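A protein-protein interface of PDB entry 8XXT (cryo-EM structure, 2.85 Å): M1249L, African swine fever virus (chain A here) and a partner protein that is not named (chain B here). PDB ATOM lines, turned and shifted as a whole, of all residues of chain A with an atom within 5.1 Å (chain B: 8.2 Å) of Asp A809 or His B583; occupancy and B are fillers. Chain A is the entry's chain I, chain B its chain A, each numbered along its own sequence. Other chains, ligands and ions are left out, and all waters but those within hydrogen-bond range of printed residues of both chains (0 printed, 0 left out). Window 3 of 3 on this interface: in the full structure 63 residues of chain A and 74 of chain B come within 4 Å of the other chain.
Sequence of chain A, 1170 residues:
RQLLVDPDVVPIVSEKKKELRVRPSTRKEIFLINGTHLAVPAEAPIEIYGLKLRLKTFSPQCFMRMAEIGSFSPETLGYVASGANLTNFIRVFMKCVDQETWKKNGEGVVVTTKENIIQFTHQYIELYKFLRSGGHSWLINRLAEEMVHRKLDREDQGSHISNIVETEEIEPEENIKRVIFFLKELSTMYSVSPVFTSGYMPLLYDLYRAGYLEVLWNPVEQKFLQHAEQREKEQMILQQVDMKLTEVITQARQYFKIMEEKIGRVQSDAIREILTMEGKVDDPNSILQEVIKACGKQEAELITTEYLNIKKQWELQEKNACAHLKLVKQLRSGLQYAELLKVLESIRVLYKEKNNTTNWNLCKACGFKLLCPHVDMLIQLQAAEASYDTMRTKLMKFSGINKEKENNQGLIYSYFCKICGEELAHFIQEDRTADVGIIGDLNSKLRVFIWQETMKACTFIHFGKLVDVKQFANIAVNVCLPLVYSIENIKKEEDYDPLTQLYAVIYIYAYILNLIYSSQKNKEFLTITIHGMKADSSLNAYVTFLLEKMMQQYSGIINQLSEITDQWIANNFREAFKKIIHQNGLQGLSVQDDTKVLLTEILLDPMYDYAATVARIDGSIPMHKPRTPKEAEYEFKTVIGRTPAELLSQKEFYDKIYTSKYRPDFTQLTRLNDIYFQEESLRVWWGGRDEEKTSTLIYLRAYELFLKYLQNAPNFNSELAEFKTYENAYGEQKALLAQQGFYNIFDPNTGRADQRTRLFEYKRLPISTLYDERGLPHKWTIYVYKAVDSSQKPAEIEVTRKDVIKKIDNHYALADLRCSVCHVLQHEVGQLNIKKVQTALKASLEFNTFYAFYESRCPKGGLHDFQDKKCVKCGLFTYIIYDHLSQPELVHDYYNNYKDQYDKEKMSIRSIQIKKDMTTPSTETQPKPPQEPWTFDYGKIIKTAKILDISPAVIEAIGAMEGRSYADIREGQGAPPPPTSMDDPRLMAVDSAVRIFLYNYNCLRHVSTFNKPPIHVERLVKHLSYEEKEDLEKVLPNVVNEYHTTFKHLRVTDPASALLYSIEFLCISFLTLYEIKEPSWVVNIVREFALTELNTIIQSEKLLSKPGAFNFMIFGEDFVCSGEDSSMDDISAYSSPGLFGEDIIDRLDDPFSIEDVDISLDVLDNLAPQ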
ATOM      1  N   TYR A 785      28.180 -30.293  20.730  1.00  0.00           N
ATOM      2  CA  TYR A 785      27.786 -31.350  19.811  1.00  0.00           C
ATOM      3  C   TYR A 785      28.435 -32.664  20.215  1.00  0.00           C
ATOM      4  O   TYR A 785      29.505 -32.686  20.824  1.00  0.00           O
ATOM      5  CB  TYR A 785      28.158 -31.001  18.368  1.00  0.00           C
ATOM      6  CG  TYR A 785      27.299 -29.909  17.785  1.00  0.00           C
ATOM      7  CD1 TYR A 785      27.473 -28.586  18.163  1.00  0.00           C
ATOM      8  CD2 TYR A 785      26.307 -30.201  16.864  1.00  0.00           C
ATOM      9  CE1 TYR A 785      26.686 -27.588  17.638  1.00  0.00           C
ATOM     10  CE2 TYR A 785      25.515 -29.211  16.336  1.00  0.00           C
ATOM     11  CZ  TYR A 785      25.710 -27.907  16.725  1.00  0.00           C
ATOM     12  OH  TYR A 785      24.924 -26.916  16.198  1.00  0.00           O
ATOM     13  N   LYS A 807      32.252 -25.626  11.304  1.00  0.00           N
ATOM     14  CA  LYS A 807      32.907 -26.769  11.927  1.00  0.00           C
ATOM     15  C   LYS A 807      32.018 -27.988  12.131  1.00  0.00           C
ATOM     16  O   LYS A 807      32.547 -29.072  12.393  1.00  0.00           O
ATOM     17  CB  LYS A 807      33.494 -26.362  13.287  1.00  0.00           C
ATOM     18  CG  LYS A 807      34.533 -25.255  13.208  1.00  0.00           C
ATOM     19  CD  LYS A 807      34.997 -24.836  14.592  1.00  0.00           C
ATOM     20  CE  LYS A 807      35.942 -23.646  14.531  1.00  0.00           C
ATOM     21  NZ  LYS A 807      37.296 -24.033  14.050  1.00  0.00           N
ATOM     22  N   ILE A 808      30.700 -27.853  12.020  1.00  0.00           N
ATOM     23  CA  ILE A 808      29.770 -28.937  12.317  1.00  0.00           C
ATOM     24  C   ILE A 808      29.150 -29.435  11.020  1.00  0.00           C
ATOM     25  O   ILE A 808      28.745 -28.637  10.167  1.00  0.00           O
ATOM     26  CB  ILE A 808      28.677 -28.491  13.305  1.00  0.00           C
ATOM     27  CG1 ILE A 808      29.301 -27.809  14.523  1.00  0.00           C
ATOM     28  CG2 ILE A 808      27.822 -29.672  13.719  1.00  0.00           C
ATOM     29  CD1 ILE A 808      30.273 -28.676  15.277  1.00  0.00           C
ATOM     30  N   ASP A 809      29.070 -30.756  10.877  1.00  0.00           N
ATOM     31  CA  ASP A 809      28.463 -31.377   9.708  1.00  0.00           C
ATOM     32  C   ASP A 809      27.607 -32.550  10.179  1.00  0.00           C
ATOM     33  O   ASP A 809      27.348 -32.714  11.375  1.00  0.00           O
ATOM     34  CB  ASP A 809      29.540 -31.788   8.694  1.00  0.00           C
ATOM     35  CG  ASP A 809      30.147 -33.139   8.999  1.00  0.00           C
ATOM     36  OD1 ASP A 809      29.572 -34.156   8.559  1.00  0.00           O
ATOM     37  OD2 ASP A 809      31.197 -33.183   9.674  1.00  0.00           O
ATOM     38  N   ASN A 810      27.162 -33.373   9.224  1.00  0.00           N
ATOM     39  CA  ASN A 810      26.231 -34.455   9.531  1.00  0.00           C
ATOM     40  C   ASN A 810      26.823 -35.499  10.466  1.00  0.00           C
ATOM     41  O   ASN A 810      26.067 -36.246  11.096  1.00  0.00           O
ATOM     42  CB  ASN A 810      25.768 -35.125   8.238  1.00  0.00           C
ATOM     43  CG  ASN A 810      24.846 -34.244   7.425  1.00  0.00           C
ATOM     44  OD1 ASN A 810      25.246 -33.182   6.949  1.00  0.00           O
ATOM     45  ND2 ASN A 810      23.602 -34.680   7.260  1.00  0.00           N
ATOM     46  N   HIS A 811      28.150 -35.573  10.576  1.00  0.00           N
ATOM     47  CA  HIS A 811      28.774 -36.581  11.423  1.00  0.00           C
ATOM     48  C   HIS A 811      28.589 -36.307  12.910  1.00  0.00           C
ATOM     49  O   HIS A 811      28.937 -37.167  13.724  1.00  0.00           O
ATOM     50  CB  HIS A 811      30.265 -36.692  11.101  1.00  0.00           C
ATOM     51  CG  HIS A 811      30.548 -37.109   9.692  1.00  0.00           C
ATOM     52  ND1 HIS A 811      29.990 -38.232   9.122  1.00  0.00           N
ATOM     53  CD2 HIS A 811      31.339 -36.560   8.740  1.00  0.00           C
ATOM     54  CE1 HIS A 811      30.418 -38.353   7.878  1.00  0.00           C
ATOM     55  NE2 HIS A 811      31.237 -37.350   7.622  1.00  0.00           N
ATOM     56  N   TYR A 812      28.065 -35.142  13.282  1.00  0.00           N
ATOM     57  CA  TYR A 812      27.814 -34.808  14.674  1.00  0.00           C
ATOM     58  C   TYR A 812      26.345 -34.453  14.856  1.00  0.00           C
ATOM     59  O   TYR A 812      25.625 -34.184  13.894  1.00  0.00           O
ATOM     60  CB  TYR A 812      28.690 -33.645  15.151  1.00  0.00           C
ATOM     61  CG  TYR A 812      30.171 -33.919  15.077  1.00  0.00           C
ATOM     62  CD1 TYR A 812      30.850 -33.863  13.870  1.00  0.00           C
ATOM     63  CD2 TYR A 812      30.889 -34.247  16.216  1.00  0.00           C
ATOM     64  CE1 TYR A 812      32.201 -34.115  13.802  1.00  0.00           C
ATOM     65  CE2 TYR A 812      32.239 -34.505  16.157  1.00  0.00           C
ATOM     66  CZ  TYR A 812      32.891 -34.435  14.950  1.00  0.00           C
ATOM     67  OH  TYR A 812      34.241 -34.688  14.890  1.00  0.00           O
ATOM     68  N   ALA A 813      25.906 -34.467  16.110  1.00  0.00           N
ATOM     69  CA  ALA A 813      24.546 -34.100  16.463  1.00  0.00           C
ATOM     70  C   ALA A 813      24.572 -33.152  17.653  1.00  0.00           C
ATOM     71  O   ALA A 813      25.457 -33.227  18.509  1.00  0.00           O
ATOM     72  CB  ALA A 813      23.691 -35.330  16.787  1.00  0.00           C
ATOM     73  N   TRP B 573      17.925 -19.481   2.202  1.00  0.00           N
ATOM     74  CA  TRP B 573      17.826 -20.777   2.866  1.00  0.00           C
ATOM     75  C   TRP B 573      18.776 -20.871   4.050  1.00  0.00           C
ATOM     76  O   TRP B 573      18.401 -21.371   5.116  1.00  0.00           O
ATOM     77  CB  TRP B 573      18.111 -21.889   1.861  1.00  0.00           C
ATOM     78  CG  TRP B 573      18.316 -23.244   2.461  1.00  0.00           C
ATOM     79  CD1 TRP B 573      19.485 -23.934   2.527  1.00  0.00           C
ATOM     80  CD2 TRP B 573      17.321 -24.084   3.054  1.00  0.00           C
ATOM     81  NE1 TRP B 573      19.286 -25.146   3.131  1.00  0.00           N
ATOM     82  CE2 TRP B 573      17.964 -25.263   3.463  1.00  0.00           C
ATOM     83  CE3 TRP B 573      15.950 -23.950   3.282  1.00  0.00           C
ATOM     84  CZ2 TRP B 573      17.285 -26.301   4.090  1.00  0.00           C
ATOM     85  CZ3 TRP B 573      15.280 -24.982   3.901  1.00  0.00           C
ATOM     86  CH2 TRP B 573      15.946 -26.142   4.298  1.00  0.00           C
ATOM     87  N   TYR B 578      18.869 -20.724  12.248  1.00  0.00           N
ATOM     88  CA  TYR B 578      18.646 -22.149  12.057  1.00  0.00           C
ATOM     89  C   TYR B 578      19.918 -22.968  12.186  1.00  0.00           C
ATOM     90  O   TYR B 578      19.842 -24.147  12.528  1.00  0.00           O
ATOM     91  CB  TYR B 578      18.038 -22.420  10.681  1.00  0.00           C
ATOM     92  CG  TYR B 578      16.705 -21.762  10.442  1.00  0.00           C
ATOM     93  CD1 TYR B 578      15.761 -21.678  11.449  1.00  0.00           C
ATOM     94  CD2 TYR B 578      16.386 -21.240   9.200  1.00  0.00           C
ATOM     95  CE1 TYR B 578      14.540 -21.083  11.229  1.00  0.00           C
ATOM     96  CE2 TYR B 578      15.168 -20.644   8.971  1.00  0.00           C
ATOM     97  CZ  TYR B 578      14.248 -20.568   9.988  1.00  0.00           C
ATOM     98  OH  TYR B 578      13.030 -19.972   9.766  1.00  0.00           O
ATOM     99  N   ALA B 579      21.075 -22.362  11.934  1.00  0.00           N
ATOM    100  CA  ALA B 579      22.314 -23.116  11.753  1.00  0.00           C
ATOM    101  C   ALA B 579      22.690 -24.048  12.901  1.00  0.00           C
ATOM    102  O   ALA B 579      23.153 -25.164  12.611  1.00  0.00           O
ATOM    103  CB  ALA B 579      23.464 -22.138  11.472  1.00  0.00           C
ATOM    104  N   PRO B 580      22.574 -23.674  14.182  1.00  0.00           N
ATOM    105  CA  PRO B 580      22.981 -24.617  15.240  1.00  0.00           C
ATOM    106  C   PRO B 580      22.256 -25.946  15.180  1.00  0.00           C
ATOM    107  O   PRO B 580      22.853 -26.998  15.439  1.00  0.00           O
ATOM    108  CB  PRO B 580      22.652 -23.856  16.524  1.00  0.00           C
ATOM    109  CG  PRO B 580      22.732 -22.450  16.146  1.00  0.00           C
ATOM    110  CD  PRO B 580      22.220 -22.363  14.750  1.00  0.00           C
ATOM    111  N   TYR B 581      20.977 -25.918  14.855  1.00  0.00           N
ATOM    112  CA  TYR B 581      20.198 -27.094  14.512  1.00  0.00           C
ATOM    113  C   TYR B 581      20.264 -27.272  13.004  1.00  0.00           C
ATOM    114  O   TYR B 581      20.857 -26.453  12.311  1.00  0.00           O
ATOM    115  CB  TYR B 581      18.770 -26.914  15.020  1.00  0.00           C
ATOM    116  CG  TYR B 581      18.720 -25.838  16.081  1.00  0.00           C
ATOM    117  CD1 TYR B 581      19.143 -26.099  17.376  1.00  0.00           C
ATOM    118  CD2 TYR B 581      18.301 -24.551  15.780  1.00  0.00           C
ATOM    119  CE1 TYR B 581      19.129 -25.121  18.343  1.00  0.00           C
ATOM    120  CE2 TYR B 581      18.285 -23.566  16.744  1.00  0.00           C
ATOM    121  CZ  TYR B 581      18.698 -23.860  18.023  1.00  0.00           C
ATOM    122  OH  TYR B 581      18.681 -22.886  18.991  1.00  0.00           O
ATOM    123  N   MET B 582      19.702 -28.376  12.505  1.00  0.00           N
ATOM    124  CA  MET B 582      19.740 -28.749  11.086  1.00  0.00           C
ATOM    125  C   MET B 582      21.155 -28.802  10.509  1.00  0.00           C
ATOM    126  O   MET B 582      22.053 -28.071  10.932  1.00  0.00           O
ATOM    127  CB  MET B 582      18.856 -27.827  10.223  1.00  0.00           C
ATOM    128  CG  MET B 582      19.412 -26.451   9.894  1.00  0.00           C
ATOM    129  SD  MET B 582      18.586 -25.564   8.571  1.00  0.00           S
ATOM    130  CE  MET B 582      17.891 -26.915   7.653  1.00  0.00           C
ATOM    131  N   HIS B 583      21.378 -29.683   9.547  1.00  0.00           N
ATOM    132  CA  HIS B 583      22.693 -29.824   8.932  1.00  0.00           C
ATOM    133  C   HIS B 583      22.636 -29.220   7.537  1.00  0.00           C
ATOM    134  O   HIS B 583      22.133 -29.836   6.597  1.00  0.00           O
ATOM    135  CB  HIS B 583      23.125 -31.284   8.920  1.00  0.00           C
ATOM    136  CG  HIS B 583      23.357 -31.841  10.289  1.00  0.00           C
ATOM    137  ND1 HIS B 583      24.321 -31.340  11.138  1.00  0.00           N
ATOM    138  CD2 HIS B 583      22.738 -32.835  10.968  1.00  0.00           C
ATOM    139  CE1 HIS B 583      24.293 -32.009  12.276  1.00  0.00           C
ATOM    140  NE2 HIS B 583      23.342 -32.923  12.199  1.00  0.00           N
ATOM    141  N   TYR B 584      23.149 -28.000   7.414  1.00  0.00           N
ATOM    142  CA  TYR B 584      23.195 -27.328   6.126  1.00  0.00           C
ATOM    143  C   TYR B 584      24.180 -28.021   5.199  1.00  0.00           C
ATOM    144  O   TYR B 584      25.303 -28.346   5.591  1.00  0.00           O
ATOM    145  CB  TYR B 584      23.604 -25.868   6.305  1.00  0.00           C
ATOM    146  CG  TYR B 584      22.462 -24.933   6.593  1.00  0.00           C
ATOM    147  CD1 TYR B 584      21.352 -24.894   5.772  1.00  0.00           C
ATOM    148  CD2 TYR B 584      22.502 -24.078   7.681  1.00  0.00           C
ATOM    149  CE1 TYR B 584      20.312 -24.039   6.028  1.00  0.00           C
ATOM    150  CE2 TYR B 584      21.464 -23.219   7.945  1.00  0.00           C
ATOM    151  CZ  TYR B 584      20.373 -23.203   7.115  1.00  0.00           C
ATOM    152  OH  TYR B 584      19.332 -22.348   7.373  1.00  0.00           O
ATOM    153  N   ASN B 585      23.759 -28.239   3.959  1.00  0.00           N
ATOM    154  CA  ASN B 585      24.658 -28.760   2.944  1.00  0.00           C
ATOM    155  C   ASN B 585      25.531 -27.627   2.421  1.00  0.00           C
ATOM    156  O   ASN B 585      25.021 -26.569   2.045  1.00  0.00           O
ATOM    157  CB  ASN B 585      23.867 -29.396   1.807  1.00  0.00           C
ATOM    158  CG  ASN B 585      24.640 -30.481   1.100  1.00  0.00           C
ATOM    159  OD1 ASN B 585      25.823 -30.328   0.811  1.00  0.00           O
ATOM    160  ND2 ASN B 585      23.974 -31.592   0.819  1.00  0.00           N
ATOM    161  N   LYS B 586      26.847 -27.848   2.403  1.00  0.00           N
ATOM    162  CA  LYS B 586      27.762 -26.791   1.989  1.00  0.00           C
ATOM    163  C   LYS B 586      27.587 -26.407   0.529  1.00  0.00           C
ATOM    164  O   LYS B 586      28.025 -25.324   0.127  1.00  0.00           O
ATOM    165  CB  LYS B 586      29.206 -27.215   2.249  1.00  0.00           C
ATOM    166  CG  LYS B 586      29.612 -27.137   3.710  1.00  0.00           C
ATOM    167  CD  LYS B 586      29.628 -25.700   4.202  1.00  0.00           C
ATOM    168  CE  LYS B 586      30.541 -24.831   3.351  1.00  0.00           C
ATOM    169  NZ  LYS B 586      30.689 -23.462   3.918  1.00  0.00           N
ATOM    170  N   ASP B 588      24.660 -25.901  -0.751  1.00  0.00           N
ATOM    171  CA  ASP B 588      23.385 -25.205  -0.804  1.00  0.00           C
ATOM    172  C   ASP B 588      23.424 -23.811  -0.198  1.00  0.00           C
ATOM    173  O   ASP B 588      22.501 -23.029  -0.436  1.00  0.00           O
ATOM    174  CB  ASP B 588      22.306 -26.017  -0.077  1.00  0.00           C
ATOM    175  CG  ASP B 588      21.831 -27.205  -0.880  1.00  0.00           C
ATOM    176  OD1 ASP B 588      22.232 -27.325  -2.055  1.00  0.00           O
ATOM    177  OD2 ASP B 588      21.056 -28.017  -0.336  1.00  0.00           O
ATOM    178  N   ILE B 589      24.460 -23.483   0.571  1.00  0.00           N
ATOM    179  CA  ILE B 589      24.491 -22.251   1.349  1.00  0.00           C
ATOM    180  C   ILE B 589      25.343 -21.175   0.690  1.00  0.00           C
ATOM    181  O   ILE B 589      25.713 -20.196   1.345  1.00  0.00           O
ATOM    182  CB  ILE B 589      24.971 -22.523   2.781  1.00  0.00           C
ATOM    183  CG1 ILE B 589      26.385 -23.095   2.764  1.00  0.00           C
ATOM    184  CG2 ILE B 589      24.031 -23.482   3.472  1.00  0.00           C
ATOM    185  CD1 ILE B 589      27.164 -22.808   4.011  1.00  0.00           C
ATOM    186  N   MET B 720      13.084 -26.939  15.812  1.00  0.00           N
ATOM    187  CA  MET B 720      13.961 -27.630  14.876  1.00  0.00           C
ATOM    188  C   MET B 720      14.187 -29.086  15.255  1.00  0.00           C
ATOM    189  O   MET B 720      14.522 -29.893  14.383  1.00  0.00           O
ATOM    190  CB  MET B 720      15.299 -26.905  14.777  1.00  0.00           C
ATOM    191  CG  MET B 720      15.236 -25.470  14.270  1.00  0.00           C
ATOM    192  SD  MET B 720      15.236 -25.276  12.473  1.00  0.00           S
ATOM    193  CE  MET B 720      13.567 -25.733  12.031  1.00  0.00           C
ATOM    194  N   PRO B 725      13.798 -30.695   8.149  1.00  0.00           N
ATOM    195  CA  PRO B 725      13.823 -29.589   7.184  1.00  0.00           C
ATOM    196  C   PRO B 725      13.803 -30.025   5.732  1.00  0.00           C
ATOM    197  O   PRO B 725      13.365 -29.251   4.873  1.00  0.00           O
ATOM    198  CB  PRO B 725      15.128 -28.869   7.531  1.00  0.00           C
ATOM    199  CG  PRO B 725      15.399 -29.238   8.938  1.00  0.00           C
ATOM    200  CD  PRO B 725      14.952 -30.650   9.057  1.00  0.00           C
ATOM    201  N   GLU B 726      14.272 -31.234   5.424  1.00  0.00           N
ATOM    202  CA  GLU B 726      14.257 -31.684   4.039  1.00  0.00           C
ATOM    203  C   GLU B 726      12.841 -31.917   3.535  1.00  0.00           C
ATOM    204  O   GLU B 726      12.582 -31.758   2.339  1.00  0.00           O
ATOM    205  CB  GLU B 726      15.088 -32.956   3.887  1.00  0.00           C
ATOM    206  CG  GLU B 726      16.581 -32.740   4.042  1.00  0.00           C
ATOM    207  CD  GLU B 726      17.396 -33.818   3.357  1.00  0.00           C
ATOM    208  OE1 GLU B 726      16.908 -34.962   3.265  1.00  0.00           O
ATOM    209  OE2 GLU B 726      18.527 -33.521   2.914  1.00  0.00           O
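A ring nitrogen (ND1) of His B583 sits close to the backbone carbonyl oxygen (O) of Asp A809 (3.3 Å). The backbone carbonyl oxygen (O) of Pro B580 sits close to the side-chain hydroxyl (OH) of Tyr A785, at 2.2 Å. A ring nitrogen (NE2) of His B583 sits close to the backbone carbonyl oxygen (O) of Tyr A812.
Printed residues of chain B within 4 Å of Tyr A785: Pro B580. Asp A809 touches one residue of chain B. Asn A810 touches just one residue of chain B: His B583. Printed residues of chain B within 4 Å of Tyr A812: His B583. Of the printed residues of chain A, Pro B580 touches Tyr A785. Of chain A, only Asp A809, Asn A810 and Tyr A812 come within 4 Å of His B583. Ile B589 touches none of the printed residues of chain A. Met B720 touches none of the printed residues of chain A. The nearest residue of chain A that does not touch His B583 is Ile A808 (4.5 Å). The nearest printed residue of chain B that does not touch Tyr A785 is Tyr B581 (4.3 Å).
OD1 of Asp A809 is in hydrogen-bond range of N of His A811.
Among the printed residues, merely in contact across the chains: Asn A810 with His B583 (3.5 Å).
Of the 8 printed residues of chain A, 4 touch a printed residue of chain B. Hydrophobic or aromatic side chains of chain A that line the printed part of chain B: Tyr A785. Hydrophobic or aromatic side chains of chain B within 4 Å of the printed part of chain A: Pro B580 and His B583. Among the printed residues, 4 pairs touch across the chains. Among the printed residues, no Asp or Glu carboxylate lies within 4 Å of a Lys or Arg side-chain nitrogen of the other chain.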
